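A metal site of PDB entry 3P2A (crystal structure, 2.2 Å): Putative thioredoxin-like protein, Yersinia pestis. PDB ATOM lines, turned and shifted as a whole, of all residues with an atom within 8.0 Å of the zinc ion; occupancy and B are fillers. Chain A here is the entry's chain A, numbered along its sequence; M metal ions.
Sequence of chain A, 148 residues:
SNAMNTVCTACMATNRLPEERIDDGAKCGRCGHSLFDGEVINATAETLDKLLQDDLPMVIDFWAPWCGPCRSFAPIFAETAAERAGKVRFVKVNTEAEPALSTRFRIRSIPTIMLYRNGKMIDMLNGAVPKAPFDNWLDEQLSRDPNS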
ATOM      1  N   VAL A   7     -27.977  -3.684   8.178  1.00  0.00           N
ATOM      2  CA  VAL A   7     -28.668  -4.907   7.781  1.00  0.00           C
ATOM      3  C   VAL A   7     -29.008  -4.853   6.307  1.00  0.00           C
ATOM      4  O   VAL A   7     -29.505  -3.836   5.818  1.00  0.00           O
ATOM      5  CB  VAL A   7     -29.946  -5.081   8.608  1.00  0.00           C
ATOM      6  CG1 VAL A   7     -30.797  -6.190   8.044  1.00  0.00           C
ATOM      7  CG2 VAL A   7     -29.587  -5.314  10.122  1.00  0.00           C
ATOM      8  N   CYS A   8     -28.708  -5.938   5.574  1.00  0.00           N
ATOM      9  CA  CYS A   8     -29.001  -5.979   4.149  1.00  0.00           C
ATOM     10  C   CYS A   8     -30.504  -6.101   3.985  1.00  0.00           C
ATOM     11  O   CYS A   8     -31.089  -7.090   4.395  1.00  0.00           O
ATOM     12  CB  CYS A   8     -28.288  -7.147   3.442  1.00  0.00           C
ATOM     13  SG  CYS A   8     -28.898  -7.291   1.726  1.00  0.00           S
ATOM     14  N   THR A   9     -31.127  -5.107   3.372  1.00  0.00           N
ATOM     15  CA  THR A   9     -32.599  -5.082   3.337  1.00  0.00           C
ATOM     16  C   THR A   9     -33.162  -6.149   2.410  1.00  0.00           C
ATOM     17  O   THR A   9     -34.384  -6.441   2.429  1.00  0.00           O
ATOM     18  CB  THR A   9     -33.145  -3.688   2.946  1.00  0.00           C
ATOM     19  OG1 THR A   9     -32.629  -3.307   1.660  1.00  0.00           O
ATOM     20  CG2 THR A   9     -32.731  -2.652   3.973  1.00  0.00           C
ATOM     21  N   ALA A  10     -32.272  -6.766   1.621  1.00  0.00           N
ATOM     22  CA  ALA A  10     -32.663  -7.826   0.710  1.00  0.00           C
ATOM     23  C   ALA A  10     -32.521  -9.231   1.329  1.00  0.00           C
ATOM     24  O   ALA A  10     -33.482  -9.978   1.324  1.00  0.00           O
ATOM     25  CB  ALA A  10     -31.920  -7.713  -0.658  1.00  0.00           C
ATOM     26  N   CYS A  11     -31.336  -9.593   1.836  1.00  0.00           N
ATOM     27  CA  CYS A  11     -31.126 -10.919   2.402  1.00  0.00           C
ATOM     28  C   CYS A  11     -31.033 -10.955   3.939  1.00  0.00           C
ATOM     29  O   CYS A  11     -30.924 -12.036   4.527  1.00  0.00           O
ATOM     30  CB  CYS A  11     -29.888 -11.617   1.764  1.00  0.00           C
ATOM     31  SG  CYS A  11     -28.338 -11.153   2.574  1.00  0.00           S
ATOM     32  N   MET A  12     -31.123  -9.790   4.587  1.00  0.00           N
ATOM     33  CA  MET A  12     -31.075  -9.631   6.061  1.00  0.00           C
ATOM     34  C   MET A  12     -29.705  -9.852   6.706  1.00  0.00           C
ATOM     35  O   MET A  12     -29.574  -9.872   7.935  1.00  0.00           O
ATOM     36  CB  MET A  12     -32.065 -10.571   6.744  1.00  0.00           C
ATOM     37  CG  MET A  12     -33.506 -10.346   6.363  1.00  0.00           C
ATOM     38  SD  MET A  12     -34.131  -8.650   7.070  1.00  0.00           S
ATOM     39  CE  MET A  12     -34.584  -7.810   5.379  1.00  0.00           C
ATOM     40  N   ALA A  13     -28.675 -10.038   5.887  1.00  0.00           N
ATOM     41  CA  ALA A  13     -27.369 -10.284   6.460  1.00  0.00           C
ATOM     42  C   ALA A  13     -26.848  -9.061   7.183  1.00  0.00           C
ATOM     43  O   ALA A  13     -27.001  -7.931   6.713  1.00  0.00           O
ATOM     44  CB  ALA A  13     -26.402 -10.658   5.363  1.00  0.00           C
ATOM     45  N   THR A  14     -26.172  -9.272   8.303  1.00  0.00           N
ATOM     46  CA  THR A  14     -25.510  -8.159   8.949  1.00  0.00           C
ATOM     47  C   THR A  14     -24.196  -7.823   8.223  1.00  0.00           C
ATOM     48  O   THR A  14     -23.406  -8.713   7.923  1.00  0.00           O
ATOM     49  CB  THR A  14     -25.250  -8.444  10.439  1.00  0.00           C
ATOM     50  OG1 THR A  14     -26.495  -8.764  11.067  1.00  0.00           O
ATOM     51  CG2 THR A  14     -24.632  -7.213  11.116  1.00  0.00           C
ATOM     52  N   ASN A  15     -24.005  -6.539   7.927  1.00  0.00           N
ATOM     53  CA  ASN A  15     -22.793  -6.045   7.257  1.00  0.00           C
ATOM     54  C   ASN A  15     -22.097  -5.035   8.110  1.00  0.00           C
ATOM     55  O   ASN A  15     -22.717  -4.047   8.506  1.00  0.00           O
ATOM     56  CB  ASN A  15     -23.126  -5.431   5.895  1.00  0.00           C
ATOM     57  CG  ASN A  15     -23.402  -6.487   4.870  1.00  0.00           C
ATOM     58  OD1 ASN A  15     -22.522  -6.846   4.072  1.00  0.00           O
ATOM     59  ND2 ASN A  15     -24.615  -7.038   4.897  1.00  0.00           N
ATOM     60  N   LYS A  27     -21.835  -2.835  -0.846  1.00  0.00           N
ATOM     61  CA  LYS A  27     -22.697  -3.913  -1.311  1.00  0.00           C
ATOM     62  C   LYS A  27     -22.763  -4.981  -0.236  1.00  0.00           C
ATOM     63  O   LYS A  27     -21.807  -5.171   0.481  1.00  0.00           O
ATOM     64  CB  LYS A  27     -22.138  -4.505  -2.595  1.00  0.00           C
ATOM     65  CG  LYS A  27     -22.114  -3.539  -3.739  1.00  0.00           C
ATOM     66  CD  LYS A  27     -23.534  -3.101  -4.103  1.00  0.00           C
ATOM     67  CE  LYS A  27     -23.667  -2.839  -5.617  1.00  0.00           C
ATOM     68  NZ  LYS A  27     -22.668  -1.863  -6.086  1.00  0.00           N
ATOM     69  N   CYS A  28     -23.889  -5.685  -0.122  1.00  0.00           N
ATOM     70  CA  CYS A  28     -23.963  -6.773   0.852  1.00  0.00           C
ATOM     71  C   CYS A  28     -22.902  -7.860   0.603  1.00  0.00           C
ATOM     72  O   CYS A  28     -22.743  -8.341  -0.502  1.00  0.00           O
ATOM     73  CB  CYS A  28     -25.352  -7.400   0.874  1.00  0.00           C
ATOM     74  SG  CYS A  28     -25.445  -8.814   1.923  1.00  0.00           S
ATOM     75  N   GLY A  29     -22.186  -8.258   1.641  1.00  0.00           N
ATOM     76  CA  GLY A  29     -21.144  -9.280   1.506  1.00  0.00           C
ATOM     77  C   GLY A  29     -21.667 -10.680   1.228  1.00  0.00           C
ATOM     78  O   GLY A  29     -20.936 -11.510   0.744  1.00  0.00           O
ATOM     79  N   ARG A  30     -22.945 -10.932   1.523  1.00  0.00           N
ATOM     80  CA  ARG A  30     -23.549 -12.227   1.247  1.00  0.00           C
ATOM     81  C   ARG A  30     -24.205 -12.197  -0.146  1.00  0.00           C
ATOM     82  O   ARG A  30     -24.153 -13.176  -0.888  1.00  0.00           O
ATOM     83  CB  ARG A  30     -24.563 -12.569   2.362  1.00  0.00           C
ATOM     84  CG  ARG A  30     -25.385 -13.886   2.228  1.00  0.00           C
ATOM     85  CD  ARG A  30     -26.441 -14.059   3.374  1.00  0.00           C
ATOM     86  NE  ARG A  30     -27.535 -15.003   3.080  1.00  0.00           N
ATOM     87  CZ  ARG A  30     -28.684 -15.086   3.768  1.00  0.00           C
ATOM     88  NH1 ARG A  30     -28.896 -14.276   4.810  1.00  0.00           N
ATOM     89  NH2 ARG A  30     -29.625 -15.974   3.430  1.00  0.00           N
ATOM     90  N   CYS A  31     -24.832 -11.091  -0.513  1.00  0.00           N
ATOM     91  CA  CYS A  31     -25.685 -11.199  -1.703  1.00  0.00           C
ATOM     92  C   CYS A  31     -25.459 -10.160  -2.798  1.00  0.00           C
ATOM     93  O   CYS A  31     -26.100 -10.236  -3.847  1.00  0.00           O
ATOM     94  CB  CYS A  31     -27.187 -11.275  -1.308  1.00  0.00           C
ATOM     95  SG  CYS A  31     -27.959  -9.643  -1.002  1.00  0.00           S
ATOM     96  N   GLY A  32     -24.597  -9.178  -2.542  1.00  0.00           N
ATOM     97  CA  GLY A  32     -24.263  -8.171  -3.552  1.00  0.00           C
ATOM     98  C   GLY A  32     -25.185  -6.973  -3.618  1.00  0.00           C
ATOM     99  O   GLY A  32     -24.932  -6.010  -4.361  1.00  0.00           O
ATOM    100  N   HIS A  33     -26.242  -7.002  -2.805  1.00  0.00           N
ATOM    101  CA  HIS A  33     -27.243  -5.930  -2.777  1.00  0.00           C
ATOM    102  C   HIS A  33     -26.704  -4.590  -2.283  1.00  0.00           C
ATOM    103  O   HIS A  33     -26.019  -4.527  -1.288  1.00  0.00           O
ATOM    104  CB  HIS A  33     -28.374  -6.359  -1.834  1.00  0.00           C
ATOM    105  CG  HIS A  33     -29.523  -5.397  -1.802  1.00  0.00           C
ATOM    106  ND1 HIS A  33     -30.273  -5.098  -2.920  1.00  0.00           N
ATOM    107  CD2 HIS A  33     -30.066  -4.695  -0.776  1.00  0.00           C
ATOM    108  CE1 HIS A  33     -31.225  -4.236  -2.591  1.00  0.00           C
ATOM    109  NE2 HIS A  33     -31.116  -3.974  -1.301  1.00  0.00           N
ATOM    110  N   SER A  34     -27.054  -3.504  -2.969  1.00  0.00           N
ATOM    111  CA  SER A  34     -26.657  -2.177  -2.525  1.00  0.00           C
ATOM    112  C   SER A  34     -27.193  -1.934  -1.126  1.00  0.00           C
ATOM    113  O   SER A  34     -28.400  -2.019  -0.882  1.00  0.00           O
ATOM    114  CB  SER A  34     -27.198  -1.144  -3.496  1.00  0.00           C
ATOM    115  OG  SER A  34     -26.834  -1.501  -4.829  1.00  0.00           O
ATOM    116  N   LEU A  35     -26.297  -1.667  -0.188  1.00  0.00           N
ATOM    117  CA  LEU A  35     -26.702  -1.513   1.188  1.00  0.00           C
ATOM    118  C   LEU A  35     -27.535  -0.228   1.435  1.00  0.00           C
ATOM    119  O   LEU A  35     -28.209  -0.114   2.447  1.00  0.00           O
ATOM    120  CB  LEU A  35     -25.489  -1.560   2.122  1.00  0.00           C
ATOM    121  CG  LEU A  35     -24.906  -2.970   2.196  1.00  0.00           C
ATOM    122  CD1 LEU A  35     -23.753  -3.005   3.198  1.00  0.00           C
ATOM    123  CD2 LEU A  35     -26.010  -3.938   2.575  1.00  0.00           C
HETATM  124 ZN    ZN M   1     -27.635  -9.266   1.368  1.00  0.00          ZN
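Within 4 Å of the zinc ion: Cys 8, Cys 11, Cys 28 and Cys 31.
The backbone NH (N) of Cys 28 is in hydrogen-bond range of the backbone carbonyl oxygen (O) of His 33 (2.7 Å).
SG of Cys 28 lies close to N of Arg 30 (3.3 Å).
The side-chain amide nitrogen (ND2) of Asn 15 lies close to the side-chain sulfur (SG) of Cys 28 (3.6 Å).
SG of Cys 11 sits close to N of Ala 13 (3.5 Å).
O of Cys 11 lies within hydrogen-bond range of NH1 of Arg 30.
N of Cys 8 sits at hydrogen-bond distance from O of Ala 13, 2.9 Å away.
The side-chain sulfur (SG) of Cys 8 lies close to the backbone NH (N) of Ala 10 (3.4 Å).
The side-chain sulfur of Cys 31 sits close to the backbone NH of His 33 (3.6 Å).
The zinc ion is bound by SG of Cys 28 (2.3 Å), SG of Cys 11 (2.3 Å), SG of Cys 8 (2.4 Å) and SG of Cys 31 (2.4 Å).
The zinc ion has four donor atoms within binding distance.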
